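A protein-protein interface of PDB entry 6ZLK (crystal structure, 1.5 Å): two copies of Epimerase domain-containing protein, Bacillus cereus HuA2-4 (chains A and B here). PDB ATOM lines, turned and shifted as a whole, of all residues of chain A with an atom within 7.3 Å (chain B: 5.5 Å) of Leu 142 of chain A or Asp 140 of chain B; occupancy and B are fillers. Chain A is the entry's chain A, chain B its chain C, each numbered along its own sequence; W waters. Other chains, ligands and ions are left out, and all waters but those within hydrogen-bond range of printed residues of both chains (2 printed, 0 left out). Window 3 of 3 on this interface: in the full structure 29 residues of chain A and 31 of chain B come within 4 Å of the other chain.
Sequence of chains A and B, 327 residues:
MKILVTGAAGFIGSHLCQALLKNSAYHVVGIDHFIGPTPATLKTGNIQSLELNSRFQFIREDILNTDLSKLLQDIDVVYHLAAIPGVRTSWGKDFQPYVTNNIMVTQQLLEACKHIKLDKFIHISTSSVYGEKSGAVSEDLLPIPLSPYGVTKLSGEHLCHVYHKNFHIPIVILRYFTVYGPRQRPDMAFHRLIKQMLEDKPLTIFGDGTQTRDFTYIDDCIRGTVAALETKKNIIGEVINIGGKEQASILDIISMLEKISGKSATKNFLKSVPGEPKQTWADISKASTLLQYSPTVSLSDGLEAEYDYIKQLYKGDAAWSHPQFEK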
ATOM      1  N   VAL A 129     -32.599 -21.663   8.560  1.00  0.00           N
ATOM      2  CA  VAL A 129     -31.216 -22.211   8.570  1.00  0.00           C
ATOM      3  C   VAL A 129     -30.280 -21.219   9.248  1.00  0.00           C
ATOM      4  O   VAL A 129     -29.225 -21.670   9.734  1.00  0.00           O
ATOM      5  CB  VAL A 129     -30.690 -22.574   7.173  1.00  0.00           C
ATOM      6  CG1 VAL A 129     -31.585 -23.592   6.453  1.00  0.00           C
ATOM      7  CG2 VAL A 129     -30.386 -21.367   6.323  1.00  0.00           C
ATOM      8  N   TYR A 130     -30.608 -19.929   9.265  1.00  0.00           N
ATOM      9  CA  TYR A 130     -29.667 -18.906   9.762  1.00  0.00           C
ATOM     10  C   TYR A 130     -29.541 -18.992  11.285  1.00  0.00           C
ATOM     11  O   TYR A 130     -28.399 -18.838  11.780  1.00  0.00           O
ATOM     12  CB  TYR A 130     -30.053 -17.505   9.361  1.00  0.00           C
ATOM     13  CG  TYR A 130     -29.852 -17.226   7.897  1.00  0.00           C
ATOM     14  CD1 TYR A 130     -28.589 -16.957   7.394  1.00  0.00           C
ATOM     15  CD2 TYR A 130     -30.910 -17.189   7.009  1.00  0.00           C
ATOM     16  CE1 TYR A 130     -28.398 -16.679   6.052  1.00  0.00           C
ATOM     17  CE2 TYR A 130     -30.736 -16.910   5.668  1.00  0.00           C
ATOM     18  CZ  TYR A 130     -29.471 -16.648   5.182  1.00  0.00           C
ATOM     19  OH  TYR A 130     -29.368 -16.423   3.843  1.00  0.00           O
ATOM     20  N   GLY A 131     -30.655 -19.166  11.993  1.00  0.00           N
ATOM     21  CA  GLY A 131     -30.650 -19.009  13.458  1.00  0.00           C
ATOM     22  C   GLY A 131     -30.712 -17.546  13.862  1.00  0.00           C
ATOM     23  O   GLY A 131     -31.448 -16.793  13.203  1.00  0.00           O
ATOM     24  N   LYS A 133     -29.250 -13.968  14.124  1.00  0.00           N
ATOM     25  CA  LYS A 133     -28.228 -13.047  13.582  1.00  0.00           C
ATOM     26  C   LYS A 133     -28.702 -11.603  13.803  1.00  0.00           C
ATOM     27  O   LYS A 133     -29.923 -11.368  13.868  1.00  0.00           O
ATOM     28  CB  LYS A 133     -27.997 -13.344  12.098  1.00  0.00           C
ATOM     29  CG  LYS A 133     -27.705 -14.810  11.756  1.00  0.00           C
ATOM     30  CD  LYS A 133     -26.269 -15.201  12.019  1.00  0.00           C
ATOM     31  CE  LYS A 133     -25.906 -16.570  11.481  1.00  0.00           C
ATOM     32  NZ  LYS A 133     -24.590 -17.030  11.993  1.00  0.00           N
ATOM     33  N   SER A 138     -27.073 -12.054   4.732  1.00  0.00           N
ATOM     34  CA  SER A 138     -26.752 -12.407   3.351  1.00  0.00           C
ATOM     35  C   SER A 138     -26.449 -13.915   3.274  1.00  0.00           C
ATOM     36  O   SER A 138     -26.177 -14.571   4.302  1.00  0.00           O
ATOM     37  CB  SER A 138     -25.672 -11.476   2.853  1.00  0.00           C
ATOM     38  OG  SER A 138     -24.502 -11.800   3.527  1.00  0.00           O
ATOM     39  N   GLU A 139     -26.444 -14.446   2.059  1.00  0.00           N
ATOM     40  CA  GLU A 139     -26.407 -15.906   1.803  1.00  0.00           C
ATOM     41  C   GLU A 139     -25.048 -16.552   2.098  1.00  0.00           C
ATOM     42  O   GLU A 139     -25.048 -17.763   2.209  1.00  0.00           O
ATOM     43  CB  GLU A 139     -26.867 -16.173   0.380  1.00  0.00           C
ATOM     44  CG  GLU A 139     -28.290 -15.689   0.140  1.00  0.00           C
ATOM     45  CD  GLU A 139     -28.476 -14.278  -0.375  1.00  0.00           C
ATOM     46  OE1 GLU A 139     -27.540 -13.428  -0.231  1.00  0.00           O
ATOM     47  OE2 GLU A 139     -29.527 -14.006  -0.949  1.00  0.00           O
ATOM     48  N   ASP A 140     -23.978 -15.766   2.301  1.00  0.00           N
ATOM     49  CA  ASP A 140     -22.623 -16.289   2.587  1.00  0.00           C
ATOM     50  C   ASP A 140     -22.411 -16.491   4.095  1.00  0.00           C
ATOM     51  O   ASP A 140     -21.358 -17.037   4.482  1.00  0.00           O
ATOM     52  CB  ASP A 140     -21.553 -15.390   1.966  1.00  0.00           C
ATOM     53  CG  ASP A 140     -21.621 -13.905   2.322  1.00  0.00           C
ATOM     54  OD1 ASP A 140     -22.657 -13.473   2.894  1.00  0.00           O
ATOM     55  OD2 ASP A 140     -20.600 -13.164   2.025  1.00  0.00           O
ATOM     56  N   LEU A 141     -23.349 -16.079   4.942  1.00  0.00           N
ATOM     57  CA  LEU A 141     -23.197 -16.183   6.410  1.00  0.00           C
ATOM     58  C   LEU A 141     -23.125 -17.645   6.844  1.00  0.00           C
ATOM     59  O   LEU A 141     -23.925 -18.500   6.351  1.00  0.00           O
ATOM     60  CB  LEU A 141     -24.376 -15.510   7.102  1.00  0.00           C
ATOM     61  CG  LEU A 141     -24.267 -14.024   7.354  1.00  0.00           C
ATOM     62  CD1 LEU A 141     -25.524 -13.596   8.079  1.00  0.00           C
ATOM     63  CD2 LEU A 141     -23.014 -13.660   8.162  1.00  0.00           C
ATOM     64  N   LEU A 142     -22.333 -17.932   7.863  1.00  0.00           N
ATOM     65  CA  LEU A 142     -22.325 -19.282   8.471  1.00  0.00           C
ATOM     66  C   LEU A 142     -23.682 -19.545   9.123  1.00  0.00           C
ATOM     67  O   LEU A 142     -24.101 -18.890  10.062  1.00  0.00           O
ATOM     68  CB  LEU A 142     -21.180 -19.408   9.481  1.00  0.00           C
ATOM     69  CG  LEU A 142     -20.436 -20.736   9.359  1.00  0.00           C
ATOM     70  CD1 LEU A 142     -19.041 -20.670   9.951  1.00  0.00           C
ATOM     71  CD2 LEU A 142     -21.258 -21.839  10.001  1.00  0.00           C
ATOM     72  N   PRO A 143     -24.446 -20.522   8.620  1.00  0.00           N
ATOM     73  CA  PRO A 143     -25.763 -20.772   9.181  1.00  0.00           C
ATOM     74  C   PRO A 143     -25.636 -21.670  10.416  1.00  0.00           C
ATOM     75  O   PRO A 143     -24.975 -22.688  10.335  1.00  0.00           O
ATOM     76  CB  PRO A 143     -26.503 -21.471   8.039  1.00  0.00           C
ATOM     77  CG  PRO A 143     -25.435 -22.134   7.220  1.00  0.00           C
ATOM     78  CD  PRO A 143     -24.152 -21.352   7.456  1.00  0.00           C
ATOM     79  N   ILE A 144     -26.314 -21.288  11.475  1.00  0.00           N
ATOM     80  CA  ILE A 144     -26.366 -22.086  12.721  1.00  0.00           C
ATOM     81  C   ILE A 144     -27.813 -22.130  13.162  1.00  0.00           C
ATOM     82  O   ILE A 144     -28.309 -21.295  13.902  1.00  0.00           O
ATOM     83  CB  ILE A 144     -25.450 -21.564  13.828  1.00  0.00           C
ATOM     84  CG1 ILE A 144     -24.033 -21.237  13.356  1.00  0.00           C
ATOM     85  CG2 ILE A 144     -25.442 -22.619  14.928  1.00  0.00           C
ATOM     86  N   PRO A 145     -28.560 -23.127  12.664  1.00  0.00           N
ATOM     87  CA  PRO A 145     -29.976 -23.184  13.005  1.00  0.00           C
ATOM     88  C   PRO A 145     -30.237 -23.230  14.513  1.00  0.00           C
ATOM     89  O   PRO A 145     -29.402 -23.732  15.294  1.00  0.00           O
ATOM     90  CB  PRO A 145     -30.397 -24.515  12.367  1.00  0.00           C
ATOM     91  CG  PRO A 145     -29.434 -24.781  11.274  1.00  0.00           C
ATOM     92  CD  PRO A 145     -28.132 -24.138  11.711  1.00  0.00           C
ATOM     93  N   LEU A 154     -31.361 -27.279   6.481  1.00  0.00           N
ATOM     94  CA  LEU A 154     -29.956 -26.999   6.122  1.00  0.00           C
ATOM     95  C   LEU A 154     -29.326 -28.282   5.560  1.00  0.00           C
ATOM     96  O   LEU A 154     -28.583 -28.178   4.594  1.00  0.00           O
ATOM     97  CB  LEU A 154     -29.205 -26.442   7.317  1.00  0.00           C
ATOM     98  CG  LEU A 154     -27.740 -26.088   7.046  1.00  0.00           C
ATOM     99  CD1 LEU A 154     -27.592 -25.128   5.881  1.00  0.00           C
ATOM    100  CD2 LEU A 154     -27.117 -25.538   8.327  1.00  0.00           C
ATOM    101  N   ARG A 175     -34.057 -19.470  -0.246  1.00  0.00           N
ATOM    102  CA  ARG A 175     -34.411 -19.388   1.188  1.00  0.00           C
ATOM    103  C   ARG A 175     -35.553 -18.406   1.366  1.00  0.00           C
ATOM    104  O   ARG A 175     -35.351 -17.164   1.340  1.00  0.00           O
ATOM    105  CB  ARG A 175     -33.214 -18.933   2.035  1.00  0.00           C
ATOM    106  CG  ARG A 175     -32.126 -19.979   2.085  1.00  0.00           C
ATOM    107  CD  ARG A 175     -30.909 -19.418   2.788  1.00  0.00           C
ATOM    108  NE  ARG A 175     -29.935 -20.484   2.959  1.00  0.00           N
ATOM    109  CZ  ARG A 175     -28.668 -20.292   3.332  1.00  0.00           C
ATOM    110  NH1 ARG A 175     -28.207 -19.091   3.570  1.00  0.00           N
ATOM    111  NH2 ARG A 175     -27.840 -21.305   3.449  1.00  0.00           N
ATOM    112  N   SER B 138      -9.611 -23.961   9.388  1.00  0.00           N
ATOM    113  CA  SER B 138      -9.994 -23.575  10.765  1.00  0.00           C
ATOM    114  C   SER B 138     -11.501 -23.766  10.973  1.00  0.00           C
ATOM    115  O   SER B 138     -12.282 -23.860   9.989  1.00  0.00           O
ATOM    116  CB  SER B 138      -9.550 -22.178  11.082  1.00  0.00           C
ATOM    117  OG  SER B 138     -10.010 -21.285  10.104  1.00  0.00           O
ATOM    118  N   GLU B 139     -11.898 -23.815  12.229  1.00  0.00           N
ATOM    119  CA  GLU B 139     -13.281 -24.193  12.593  1.00  0.00           C
ATOM    120  C   GLU B 139     -14.277 -23.062  12.271  1.00  0.00           C
ATOM    121  O   GLU B 139     -15.496 -23.303  12.459  1.00  0.00           O
ATOM    122  CB  GLU B 139     -13.305 -24.577  14.066  1.00  0.00           C
ATOM    123  CG  GLU B 139     -12.358 -25.730  14.406  1.00  0.00           C
ATOM    124  CD  GLU B 139     -10.943 -25.329  14.825  1.00  0.00           C
ATOM    125  OE1 GLU B 139     -10.491 -24.205  14.474  1.00  0.00           O
ATOM    126  OE2 GLU B 139     -10.239 -26.195  15.443  1.00  0.00           O
ATOM    127  N   ASP B 140     -13.832 -21.868  11.921  1.00  0.00           N
ATOM    128  CA  ASP B 140     -14.788 -20.778  11.576  1.00  0.00           C
ATOM    129  C   ASP B 140     -15.123 -20.793  10.079  1.00  0.00           C
ATOM    130  O   ASP B 140     -15.967 -19.970   9.663  1.00  0.00           O
ATOM    131  CB  ASP B 140     -14.269 -19.399  11.969  1.00  0.00           C
ATOM    132  CG  ASP B 140     -12.967 -18.997  11.320  1.00  0.00           C
ATOM    133  OD1 ASP B 140     -12.235 -19.886  10.825  1.00  0.00           O
ATOM    134  OD2 ASP B 140     -12.692 -17.771  11.326  1.00  0.00           O
ATOM    135  N   LEU B 141     -14.511 -21.670   9.291  1.00  0.00           N
ATOM    136  CA  LEU B 141     -14.816 -21.762   7.836  1.00  0.00           C
ATOM    137  C   LEU B 141     -16.217 -22.331   7.622  1.00  0.00           C
ATOM    138  O   LEU B 141     -16.633 -23.285   8.287  1.00  0.00           O
ATOM    139  CB  LEU B 141     -13.816 -22.648   7.109  1.00  0.00           C
ATOM    140  CG  LEU B 141     -12.400 -22.106   7.001  1.00  0.00           C
ATOM    141  CD1 LEU B 141     -11.615 -23.001   6.054  1.00  0.00           C
ATOM    142  CD2 LEU B 141     -12.370 -20.644   6.533  1.00  0.00           C
ATOM    143  N   LEU B 142     -16.934 -21.764   6.678  1.00  0.00           N
ATOM    144  CA  LEU B 142     -18.282 -22.271   6.340  1.00  0.00           C
ATOM    145  C   LEU B 142     -18.146 -23.674   5.766  1.00  0.00           C
ATOM    146  O   LEU B 142     -17.467 -23.911   4.751  1.00  0.00           O
ATOM    147  CB  LEU B 142     -18.913 -21.307   5.335  1.00  0.00           C
ATOM    148  CG  LEU B 142     -20.444 -21.325   5.324  1.00  0.00           C
ATOM    149  CD1 LEU B 142     -20.976 -19.964   4.872  1.00  0.00           C
ATOM    150  CD2 LEU B 142     -20.905 -22.432   4.415  1.00  0.00           C
ATOM    151  N   PRO B 143     -18.725 -24.702   6.432  1.00  0.00           N
ATOM    152  CA  PRO B 143     -18.570 -26.080   5.987  1.00  0.00           C
ATOM    153  C   PRO B 143     -19.591 -26.435   4.900  1.00  0.00           C
ATOM    154  O   PRO B 143     -20.775 -26.174   5.072  1.00  0.00           O
ATOM    155  CB  PRO B 143     -18.829 -26.891   7.271  1.00  0.00           C
ATOM    156  CG  PRO B 143     -19.742 -26.031   8.096  1.00  0.00           C
ATOM    157  CD  PRO B 143     -19.545 -24.590   7.654  1.00  0.00           C
ATOM    158  N   HIS B 158     -24.940 -29.618  14.101  1.00  0.00           N
ATOM    159  CA  HIS B 158     -25.976 -28.562  14.208  1.00  0.00           C
ATOM    160  C   HIS B 158     -26.988 -28.953  15.288  1.00  0.00           C
ATOM    161  O   HIS B 158     -27.453 -28.018  16.005  1.00  0.00           O
ATOM    162  CB  HIS B 158     -26.630 -28.314  12.848  1.00  0.00           C
ATOM    163  CG  HIS B 158     -25.712 -27.536  11.968  1.00  0.00           C
ATOM    164  ND1 HIS B 158     -25.568 -27.799  10.634  1.00  0.00           N
ATOM    165  CD2 HIS B 158     -24.997 -26.424  12.188  1.00  0.00           C
ATOM    166  CE1 HIS B 158     -24.701 -26.939  10.127  1.00  0.00           C
ATOM    167  NE2 HIS B 158     -24.336 -26.140  11.012  1.00  0.00           N
HETATM  168  O   HOH W   1     -27.399 -25.596  14.591  1.00  0.00           O
HETATM  169  O   HOH W   2     -22.986 -24.747   9.103  1.00  0.00           O
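Water W2 bridges a ring nitrogen (NE2) of His 158 of chain B (2.7 Å) and the backbone carbonyl oxygen of Pro 143 of chain A (3.1 Å).
Water W1 bridges O of His 158 of chain B and O of Pro 145 of chain A.
The side-chain carboxylate (OD1) of Asp 140 of chain B sits at hydrogen-bond distance from the side-chain hydroxyl (OG) of Ser 138 of chain B, at 2.7 Å.
NZ of Lys 133 of chain A is in hydrogen-bond range of O of Leu 142 of chain A, at 2.7 Å.
The side-chain hydroxyl (OG) of Ser 138 of chain A sits at hydrogen-bond distance from the side-chain carboxylate (OD1) of Asp 140 of chain A (2.6 Å).
Of the 7 printed residues of chain B, 4 touch a printed residue of chain A.
Hydrophobic or aromatic side chains of chain B within 4 Å of the printed part of chain A: Leu 142 and His 158.
Hydrophobic or aromatic side chains of chain A within 4 Å of the printed part of chain B: Leu 142, Pro 145 and Leu 154.
Along chain A the printed residues that touch a printed residue of chain B span positions 140 to 154.
Printed residues of chain B within 4 Å of Asp 140 of chain A: Leu 142.
Printed residues of chain B within 4 Å of Pro 145 of chain A: His 158.
The nearest printed residue of chain A that does not touch Asp 140 of chain B is Asp 140 of chain A (8.0 Å).
Leu 142 of chain B touches Asp 140 of chain A.
Leu 142 of chain B touches Leu 141 of chain A.
Leu 142 of chain A touches Asp 140 of chain B.
CD1 of Leu 142 of chain A touches O of Leu 141 of chain B (3.9 Å).
Leu 142 of chain A touches Leu 142 of chain B.
O of Pro 143 of chain A touches NE2 of His 158 of chain B (3.6 Å).
His 158 of chain B touches Pro 145 of chain A.
His 158 of chain B touches Leu 154 of chain A.
Asp 140 of chain A touches Leu 142 of chain B, and with the chains exchanged Leu 142 of chain A touches Asp 140 of chain B.
Leu 141 of chain A touches Leu 142 of chain B, and with the chains exchanged Leu 142 of chain A touches Leu 141 of chain B.
Leu 142 of chain A touches its own counterpart, Leu 142 of chain B.
6 positions are printed for both chains.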
